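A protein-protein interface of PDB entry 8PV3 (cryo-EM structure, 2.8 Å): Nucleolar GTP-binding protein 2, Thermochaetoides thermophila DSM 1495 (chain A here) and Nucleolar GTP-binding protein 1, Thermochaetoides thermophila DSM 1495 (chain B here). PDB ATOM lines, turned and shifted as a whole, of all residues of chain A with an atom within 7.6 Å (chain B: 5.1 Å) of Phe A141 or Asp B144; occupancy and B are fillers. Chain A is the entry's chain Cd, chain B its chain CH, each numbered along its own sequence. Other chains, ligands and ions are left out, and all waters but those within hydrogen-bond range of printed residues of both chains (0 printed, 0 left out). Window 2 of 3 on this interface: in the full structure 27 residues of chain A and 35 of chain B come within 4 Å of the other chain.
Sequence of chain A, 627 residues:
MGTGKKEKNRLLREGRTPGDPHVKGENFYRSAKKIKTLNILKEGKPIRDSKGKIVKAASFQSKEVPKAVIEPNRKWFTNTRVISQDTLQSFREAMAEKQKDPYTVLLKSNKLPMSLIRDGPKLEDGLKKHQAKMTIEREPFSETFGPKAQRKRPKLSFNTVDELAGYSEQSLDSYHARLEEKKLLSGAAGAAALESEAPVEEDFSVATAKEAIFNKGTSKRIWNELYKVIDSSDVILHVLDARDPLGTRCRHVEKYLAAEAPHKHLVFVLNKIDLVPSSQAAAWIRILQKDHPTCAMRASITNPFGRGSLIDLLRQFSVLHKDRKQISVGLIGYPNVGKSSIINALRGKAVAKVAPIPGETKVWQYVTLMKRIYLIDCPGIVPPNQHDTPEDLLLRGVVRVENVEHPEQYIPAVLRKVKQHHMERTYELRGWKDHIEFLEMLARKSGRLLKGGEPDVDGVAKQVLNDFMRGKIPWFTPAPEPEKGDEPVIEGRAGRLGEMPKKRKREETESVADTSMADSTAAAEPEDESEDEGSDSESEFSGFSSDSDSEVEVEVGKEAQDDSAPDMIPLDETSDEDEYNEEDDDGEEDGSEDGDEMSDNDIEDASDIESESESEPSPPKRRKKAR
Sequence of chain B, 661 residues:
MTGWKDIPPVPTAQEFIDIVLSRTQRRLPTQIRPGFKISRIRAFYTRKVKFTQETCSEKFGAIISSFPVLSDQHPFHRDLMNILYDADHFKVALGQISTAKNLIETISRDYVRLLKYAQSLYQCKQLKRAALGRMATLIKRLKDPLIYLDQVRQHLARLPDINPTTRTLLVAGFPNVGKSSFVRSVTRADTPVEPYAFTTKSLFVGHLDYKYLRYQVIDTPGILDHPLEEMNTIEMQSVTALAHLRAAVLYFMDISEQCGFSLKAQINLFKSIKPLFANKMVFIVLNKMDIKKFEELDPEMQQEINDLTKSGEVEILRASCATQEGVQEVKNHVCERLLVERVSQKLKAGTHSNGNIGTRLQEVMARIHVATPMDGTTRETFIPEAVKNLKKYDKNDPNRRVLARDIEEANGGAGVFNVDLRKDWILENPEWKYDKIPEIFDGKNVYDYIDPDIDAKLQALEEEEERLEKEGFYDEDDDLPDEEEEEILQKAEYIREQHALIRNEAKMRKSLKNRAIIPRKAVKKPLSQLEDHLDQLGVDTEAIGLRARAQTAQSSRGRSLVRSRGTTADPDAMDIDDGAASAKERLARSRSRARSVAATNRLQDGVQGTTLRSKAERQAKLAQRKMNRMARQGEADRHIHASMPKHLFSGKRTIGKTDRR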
ATOM      1  N   ALA A 132      19.975  24.175  27.299  1.00  0.00           N
ATOM      2  CA  ALA A 132      18.865  23.700  26.474  1.00  0.00           C
ATOM      3  C   ALA A 132      17.624  24.569  26.649  1.00  0.00           C
ATOM      4  O   ALA A 132      17.028  25.029  25.665  1.00  0.00           O
ATOM      5  CB  ALA A 132      18.552  22.244  26.816  1.00  0.00           C
ATOM      6  N   THR A 135      18.221  28.008  25.061  1.00  0.00           N
ATOM      7  CA  THR A 135      18.056  28.029  23.611  1.00  0.00           C
ATOM      8  C   THR A 135      16.589  27.940  23.219  1.00  0.00           C
ATOM      9  O   THR A 135      16.165  28.579  22.251  1.00  0.00           O
ATOM     10  CB  THR A 135      18.840  26.890  22.958  1.00  0.00           C
ATOM     11  OG1 THR A 135      18.488  25.645  23.571  1.00  0.00           O
ATOM     12  CG2 THR A 135      20.339  27.124  23.083  1.00  0.00           C
ATOM     13  N   ILE A 136      15.799  27.152  23.954  1.00  0.00           N
ATOM     14  CA  ILE A 136      14.373  27.062  23.636  1.00  0.00           C
ATOM     15  C   ILE A 136      13.658  28.377  23.943  1.00  0.00           C
ATOM     16  O   ILE A 136      12.772  28.798  23.188  1.00  0.00           O
ATOM     17  CB  ILE A 136      13.734  25.867  24.370  1.00  0.00           C
ATOM     18  CG1 ILE A 136      14.386  24.564  23.917  1.00  0.00           C
ATOM     19  CG2 ILE A 136      12.246  25.782  24.096  1.00  0.00           C
ATOM     20  CD1 ILE A 136      14.402  24.376  22.417  1.00  0.00           C
ATOM     21  N   GLU A 137      14.036  29.058  25.028  1.00  0.00           N
ATOM     22  CA  GLU A 137      13.457  30.367  25.320  1.00  0.00           C
ATOM     23  C   GLU A 137      13.862  31.404  24.280  1.00  0.00           C
ATOM     24  O   GLU A 137      13.058  32.270  23.918  1.00  0.00           O
ATOM     25  CB  GLU A 137      13.868  30.829  26.718  1.00  0.00           C
ATOM     26  CG  GLU A 137      13.128  30.133  27.843  1.00  0.00           C
ATOM     27  CD  GLU A 137      13.711  30.449  29.204  1.00  0.00           C
ATOM     28  OE1 GLU A 137      14.845  30.969  29.258  1.00  0.00           O
ATOM     29  OE2 GLU A 137      13.036  30.180  30.220  1.00  0.00           O
ATOM     30  N   GLU A 139      14.734  30.763  21.033  1.00  0.00           N
ATOM     31  CA  GLU A 139      14.147  30.382  19.750  1.00  0.00           C
ATOM     32  C   GLU A 139      13.200  29.215  19.995  1.00  0.00           C
ATOM     33  O   GLU A 139      13.661  28.084  20.231  1.00  0.00           O
ATOM     34  CB  GLU A 139      15.229  30.000  18.748  1.00  0.00           C
ATOM     35  CG  GLU A 139      16.157  31.141  18.362  1.00  0.00           C
ATOM     36  CD  GLU A 139      17.299  30.691  17.473  1.00  0.00           C
ATOM     37  OE1 GLU A 139      17.443  29.471  17.258  1.00  0.00           O
ATOM     38  OE2 GLU A 139      18.059  31.560  16.997  1.00  0.00           O
ATOM     39  N   PRO A 140      11.887  29.442  19.963  1.00  0.00           N
ATOM     40  CA  PRO A 140      10.946  28.348  20.234  1.00  0.00           C
ATOM     41  C   PRO A 140      10.922  27.324  19.109  1.00  0.00           C
ATOM     42  O   PRO A 140      11.479  27.534  18.031  1.00  0.00           O
ATOM     43  CB  PRO A 140       9.594  29.058  20.366  1.00  0.00           C
ATOM     44  CG  PRO A 140       9.789  30.412  19.812  1.00  0.00           C
ATOM     45  CD  PRO A 140      11.229  30.755  19.932  1.00  0.00           C
ATOM     46  N   PHE A 141      10.267  26.193  19.386  1.00  0.00           N
ATOM     47  CA  PHE A 141      10.190  25.114  18.406  1.00  0.00           C
ATOM     48  C   PHE A 141       9.342  25.511  17.205  1.00  0.00           C
ATOM     49  O   PHE A 141       9.628  25.106  16.074  1.00  0.00           O
ATOM     50  CB  PHE A 141       9.624  23.854  19.056  1.00  0.00           C
ATOM     51  CG  PHE A 141      10.640  23.046  19.809  1.00  0.00           C
ATOM     52  CD1 PHE A 141      11.706  22.464  19.151  1.00  0.00           C
ATOM     53  CD2 PHE A 141      10.521  22.863  21.173  1.00  0.00           C
ATOM     54  CE1 PHE A 141      12.634  21.718  19.843  1.00  0.00           C
ATOM     55  CE2 PHE A 141      11.449  22.120  21.868  1.00  0.00           C
ATOM     56  CZ  PHE A 141      12.503  21.546  21.203  1.00  0.00           C
ATOM     57  N   SER A 142       8.290  26.298  17.432  1.00  0.00           N
ATOM     58  CA  SER A 142       7.380  26.656  16.351  1.00  0.00           C
ATOM     59  C   SER A 142       7.971  27.691  15.406  1.00  0.00           C
ATOM     60  O   SER A 142       7.590  27.724  14.231  1.00  0.00           O
ATOM     61  CB  SER A 142       6.061  27.172  16.924  1.00  0.00           C
ATOM     62  OG  SER A 142       6.275  28.291  17.761  1.00  0.00           O
ATOM     63  N   GLU A 143       8.882  28.535  15.882  1.00  0.00           N
ATOM     64  CA  GLU A 143       9.499  29.541  15.029  1.00  0.00           C
ATOM     65  C   GLU A 143      10.729  29.023  14.304  1.00  0.00           C
ATOM     66  O   GLU A 143      11.289  29.736  13.464  1.00  0.00           O
ATOM     67  CB  GLU A 143       9.879  30.774  15.850  1.00  0.00           C
ATOM     68  CG  GLU A 143       8.696  31.528  16.422  1.00  0.00           C
ATOM     69  CD  GLU A 143       9.120  32.728  17.245  1.00  0.00           C
ATOM     70  OE1 GLU A 143      10.334  33.014  17.296  1.00  0.00           O
ATOM     71  OE2 GLU A 143       8.239  33.383  17.841  1.00  0.00           O
ATOM     72  N   THR A 144      11.164  27.802  14.609  1.00  0.00           N
ATOM     73  CA  THR A 144      12.352  27.259  13.961  1.00  0.00           C
ATOM     74  C   THR A 144      12.001  26.515  12.681  1.00  0.00           C
ATOM     75  O   THR A 144      12.508  26.843  11.603  1.00  0.00           O
ATOM     76  CB  THR A 144      13.091  26.333  14.920  1.00  0.00           C
ATOM     77  OG1 THR A 144      13.361  27.028  16.143  1.00  0.00           O
ATOM     78  CG2 THR A 144      14.389  25.877  14.305  1.00  0.00           C
ATOM     79  N   PHE A 145      11.138  25.509  12.780  1.00  0.00           N
ATOM     80  CA  PHE A 145      10.782  24.689  11.635  1.00  0.00           C
ATOM     81  C   PHE A 145       9.293  24.393  11.695  1.00  0.00           C
ATOM     82  O   PHE A 145       8.741  24.138  12.767  1.00  0.00           O
ATOM     83  CB  PHE A 145      11.594  23.389  11.608  1.00  0.00           C
ATOM     84  CG  PHE A 145      11.552  22.672  10.292  1.00  0.00           C
ATOM     85  CD1 PHE A 145      12.341  23.092   9.236  1.00  0.00           C
ATOM     86  CD2 PHE A 145      10.730  21.575  10.113  1.00  0.00           C
ATOM     87  CE1 PHE A 145      12.306  22.434   8.025  1.00  0.00           C
ATOM     88  CE2 PHE A 145      10.690  20.913   8.904  1.00  0.00           C
ATOM     89  CZ  PHE A 145      11.480  21.343   7.860  1.00  0.00           C
ATOM     90  N   GLY A 146       8.645  24.437  10.535  1.00  0.00           N
ATOM     91  CA  GLY A 146       7.233  24.163  10.445  1.00  0.00           C
ATOM     92  C   GLY A 146       6.497  25.164   9.579  1.00  0.00           C
ATOM     93  O   GLY A 146       7.105  25.996   8.900  1.00  0.00           O
ATOM     94  N   LYS A 148       4.702  27.716  10.495  1.00  0.00           N
ATOM     95  CA  LYS A 148       4.794  29.076  11.014  1.00  0.00           C
ATOM     96  C   LYS A 148       6.231  29.465  11.336  1.00  0.00           C
ATOM     97  O   LYS A 148       6.457  30.339  12.178  1.00  0.00           O
ATOM     98  CB  LYS A 148       3.918  29.241  12.257  1.00  0.00           C
ATOM     99  CG  LYS A 148       2.473  28.811  12.077  1.00  0.00           C
ATOM    100  CD  LYS A 148       1.817  29.509  10.899  1.00  0.00           C
ATOM    101  CE  LYS A 148       0.436  28.936  10.629  1.00  0.00           C
ATOM    102  NZ  LYS A 148      -0.187  29.537   9.422  1.00  0.00           N
ATOM    103  N   ALA A 149       7.205  28.830  10.690  1.00  0.00           N
ATOM    104  CA  ALA A 149       8.603  29.073  11.008  1.00  0.00           C
ATOM    105  C   ALA A 149       9.054  30.433  10.492  1.00  0.00           C
ATOM    106  O   ALA A 149       8.656  30.881   9.413  1.00  0.00           O
ATOM    107  CB  ALA A 149       9.483  27.976  10.415  1.00  0.00           C
ATOM    108  N   HIS B  89      18.029  22.499  18.348  1.00  0.00           N
ATOM    109  CA  HIS B  89      16.619  22.193  18.570  1.00  0.00           C
ATOM    110  C   HIS B  89      16.339  20.706  18.389  1.00  0.00           C
ATOM    111  O   HIS B  89      15.581  20.109  19.162  1.00  0.00           O
ATOM    112  CB  HIS B  89      15.763  23.021  17.614  1.00  0.00           C
ATOM    113  CG  HIS B  89      15.530  24.425  18.073  1.00  0.00           C
ATOM    114  ND1 HIS B  89      16.494  25.405  17.979  1.00  0.00           N
ATOM    115  CD2 HIS B  89      14.443  25.019  18.617  1.00  0.00           C
ATOM    116  CE1 HIS B  89      16.014  26.539  18.453  1.00  0.00           C
ATOM    117  NE2 HIS B  89      14.772  26.332  18.847  1.00  0.00           N
ATOM    118  N   VAL B  92      17.822  18.869  21.421  1.00  0.00           N
ATOM    119  CA  VAL B  92      17.040  19.153  22.623  1.00  0.00           C
ATOM    120  C   VAL B  92      15.702  18.420  22.586  1.00  0.00           C
ATOM    121  O   VAL B  92      15.255  17.879  23.603  1.00  0.00           O
ATOM    122  CB  VAL B  92      16.868  20.674  22.804  1.00  0.00           C
ATOM    123  CG1 VAL B  92      15.827  20.991  23.859  1.00  0.00           C
ATOM    124  CG2 VAL B  92      18.179  21.284  23.250  1.00  0.00           C
ATOM    125  N   ALA B  93      15.062  18.358  21.415  1.00  0.00           N
ATOM    126  CA  ALA B  93      13.793  17.642  21.297  1.00  0.00           C
ATOM    127  C   ALA B  93      13.967  16.153  21.576  1.00  0.00           C
ATOM    128  O   ALA B  93      13.197  15.555  22.343  1.00  0.00           O
ATOM    129  CB  ALA B  93      13.200  17.865  19.907  1.00  0.00           C
ATOM    130  N   GLN B  96      14.640  15.602  25.263  1.00  0.00           N
ATOM    131  CA  GLN B  96      13.413  15.680  26.050  1.00  0.00           C
ATOM    132  C   GLN B  96      12.597  14.404  25.924  1.00  0.00           C
ATOM    133  O   GLN B  96      11.993  13.951  26.906  1.00  0.00           O
ATOM    134  CB  GLN B  96      12.585  16.889  25.628  1.00  0.00           C
ATOM    135  CG  GLN B  96      13.184  18.214  26.041  1.00  0.00           C
ATOM    136  CD  GLN B  96      12.214  19.359  25.889  1.00  0.00           C
ATOM    137  OE1 GLN B  96      11.002  19.160  25.873  1.00  0.00           O
ATOM    138  NE2 GLN B  96      12.742  20.568  25.767  1.00  0.00           N
ATOM    139  N   LEU B 142       5.391  17.752  26.711  1.00  0.00           N
ATOM    140  CA  LEU B 142       6.105  17.580  25.453  1.00  0.00           C
ATOM    141  C   LEU B 142       5.300  18.021  24.239  1.00  0.00           C
ATOM    142  O   LEU B 142       5.406  17.383  23.190  1.00  0.00           O
ATOM    143  CB  LEU B 142       6.507  16.118  25.258  1.00  0.00           C
ATOM    144  CG  LEU B 142       7.537  15.454  26.160  1.00  0.00           C
ATOM    145  CD1 LEU B 142       7.562  13.974  25.859  1.00  0.00           C
ATOM    146  CD2 LEU B 142       8.903  16.069  25.954  1.00  0.00           C
ATOM    147  N   LYS B 143       4.499  19.081  24.351  1.00  0.00           N
ATOM    148  CA  LYS B 143       3.590  19.444  23.266  1.00  0.00           C
ATOM    149  C   LYS B 143       4.341  19.950  22.036  1.00  0.00           C
ATOM    150  O   LYS B 143       4.026  19.573  20.902  1.00  0.00           O
ATOM    151  CB  LYS B 143       2.597  20.493  23.761  1.00  0.00           C
ATOM    152  CG  LYS B 143       1.591  20.937  22.720  1.00  0.00           C
ATOM    153  CD  LYS B 143       0.642  21.976  23.284  1.00  0.00           C
ATOM    154  CE  LYS B 143      -0.516  22.227  22.337  1.00  0.00           C
ATOM    155  NZ  LYS B 143      -0.042  22.736  21.023  1.00  0.00           N
ATOM    156  N   ASP B 144       5.343  20.807  22.244  1.00  0.00           N
ATOM    157  CA  ASP B 144       6.053  21.404  21.112  1.00  0.00           C
ATOM    158  C   ASP B 144       7.102  20.488  20.478  1.00  0.00           C
ATOM    159  O   ASP B 144       7.205  20.487  19.234  1.00  0.00           O
ATOM    160  CB  ASP B 144       6.653  22.749  21.534  1.00  0.00           C
ATOM    161  CG  ASP B 144       5.621  23.690  22.116  1.00  0.00           C
ATOM    162  OD1 ASP B 144       4.424  23.534  21.796  1.00  0.00           O
ATOM    163  OD2 ASP B 144       6.004  24.585  22.895  1.00  0.00           O
ATOM    164  N   PRO B 145       7.936  19.729  21.232  1.00  0.00           N
ATOM    165  CA  PRO B 145       8.875  18.816  20.554  1.00  0.00           C
ATOM    166  C   PRO B 145       8.225  17.771  19.663  1.00  0.00           C
ATOM    167  O   PRO B 145       8.823  17.396  18.653  1.00  0.00           O
ATOM    168  CB  PRO B 145       9.619  18.159  21.722  1.00  0.00           C
ATOM    169  CG  PRO B 145       9.615  19.164  22.759  1.00  0.00           C
ATOM    170  CD  PRO B 145       8.286  19.829  22.668  1.00  0.00           C
ATOM    171  N   LEU B 146       7.022  17.302  19.991  1.00  0.00           N
ATOM    172  CA  LEU B 146       6.375  16.292  19.159  1.00  0.00           C
ATOM    173  C   LEU B 146       5.956  16.873  17.811  1.00  0.00           C
ATOM    174  O   LEU B 146       6.125  16.231  16.768  1.00  0.00           O
ATOM    175  CB  LEU B 146       5.182  15.696  19.900  1.00  0.00           C
ATOM    176  CG  LEU B 146       5.563  14.864  21.128  1.00  0.00           C
ATOM    177  CD1 LEU B 146       4.334  14.379  21.870  1.00  0.00           C
ATOM    178  CD2 LEU B 146       6.453  13.699  20.744  1.00  0.00           C
ATOM    179  N   ILE B 147       5.424  18.099  17.816  1.00  0.00           N
ATOM    180  CA  ILE B 147       5.075  18.782  16.571  1.00  0.00           C
ATOM    181  C   ILE B 147       6.322  19.045  15.736  1.00  0.00           C
ATOM    182  O   ILE B 147       6.340  18.810  14.514  1.00  0.00           O
ATOM    183  CB  ILE B 147       4.322  20.089  16.882  1.00  0.00           C
ATOM    184  CG1 ILE B 147       3.050  19.803  17.677  1.00  0.00           C
ATOM    185  CG2 ILE B 147       3.988  20.837  15.608  1.00  0.00           C
ATOM    186  CD1 ILE B 147       2.454  21.029  18.317  1.00  0.00           C
ATOM    187  N   TYR B 148       7.388  19.524  16.391  1.00  0.00           N
ATOM    188  CA  TYR B 148       8.638  19.802  15.690  1.00  0.00           C
ATOM    189  C   TYR B 148       9.213  18.535  15.072  1.00  0.00           C
ATOM    190  O   TYR B 148       9.637  18.540  13.911  1.00  0.00           O
ATOM    191  CB  TYR B 148       9.636  20.443  16.657  1.00  0.00           C
ATOM    192  CG  TYR B 148      11.048  20.584  16.127  1.00  0.00           C
ATOM    193  CD1 TYR B 148      11.394  21.645  15.304  1.00  0.00           C
ATOM    194  CD2 TYR B 148      12.040  19.675  16.475  1.00  0.00           C
ATOM    195  CE1 TYR B 148      12.677  21.785  14.824  1.00  0.00           C
ATOM    196  CE2 TYR B 148      13.325  19.807  15.996  1.00  0.00           C
ATOM    197  CZ  TYR B 148      13.637  20.863  15.174  1.00  0.00           C
ATOM    198  OH  TYR B 148      14.921  20.999  14.699  1.00  0.00           O
ATOM    199  N   LEU B 149       9.188  17.428  15.815  1.00  0.00           N
ATOM    200  CA  LEU B 149       9.761  16.187  15.317  1.00  0.00           C
ATOM    201  C   LEU B 149       8.904  15.559  14.230  1.00  0.00           C
ATOM    202  O   LEU B 149       9.443  14.900  13.341  1.00  0.00           O
ATOM    203  CB  LEU B 149       9.973  15.207  16.468  1.00  0.00           C
ATOM    204  CG  LEU B 149      11.187  15.501  17.350  1.00  0.00           C
ATOM    205  CD1 LEU B 149      11.217  14.569  18.541  1.00  0.00           C
ATOM    206  CD2 LEU B 149      12.476  15.405  16.556  1.00  0.00           C
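NE2 of His B89 lies within hydrogen-bond range of O of Glu A139, 2.5 Å away.
A ring nitrogen (NE2) of His B89 is in hydrogen-bond range of the side-chain hydroxyl of Thr A144 (3.1 Å).
O of Ala A132 sits at hydrogen-bond distance from OG1 of Thr A135, at 2.6 Å.
The side-chain hydroxyl (OG1) of Thr A144 lies within hydrogen-bond range of the backbone carbonyl oxygen (O) of Pro A140, at 2.7 Å.
Printed residues of chain B that touch a printed residue of chain A: His B89, Val B92, Ala B93, Asp B144, Pro B145 and Tyr B148.
Hydrophobic or aromatic side chains of chain B that line the printed part of chain A: His B89, Val B92, Ala B93, Pro B145 and Tyr B148.
Along chain A the printed residues that touch a printed residue of chain B span positions 132 to 145.
Of the printed residues of chain B, Ile A136 touches His B89 (3.9 Å) and Val B92 (3.9 Å).
Of the printed residues of chain B, Glu A139 touches His B89.
Of chain B, only His B89, Ala B93, Asp B144, Pro B145 and Tyr B148 come within 4 Å of Phe A141.
Lys A148 touches none of the printed residues of chain B.
Printed residues of chain A within 4 Å of Ala B93: Phe A141.
Asp B144 touches just one residue of chain A: Phe A141.
Of the printed residues of chain A, Pro B145 touches Phe A141 (3.6 Å).
Printed residues of chain A within 4 Å of Tyr B148: Phe A141 (3.6 Å) and Phe A145 (3.8 Å).
The nearest residue of chain B that does not touch Phe A141 is Val B92 (4.3 Å).
The nearest residue of chain A that does not touch Asp B144 is Ser A142 (5.7 Å).
The nearest printed residue of chain B that does not touch Ile A136 is Gln B96 (4.7 Å).
Among the printed residues, pairs that only touch across the chains: Ala A132 with Val B92 (3.7 Å), Ile A136 with His B89 (3.9 Å), Ile A136 with Val B92 (3.9 Å), Pro A140 with His B89 (3.6 Å), Phe A141 with His B89 (3.4 Å), Phe A141 with Ala B93 (3.9 Å), Phe A141 with Asp B144 (3.9 Å), Phe A141 with Pro B145 (3.6 Å), Phe A141 with Tyr B148 (3.6 Å) and Phe A145 with Tyr B148 (3.8 Å).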
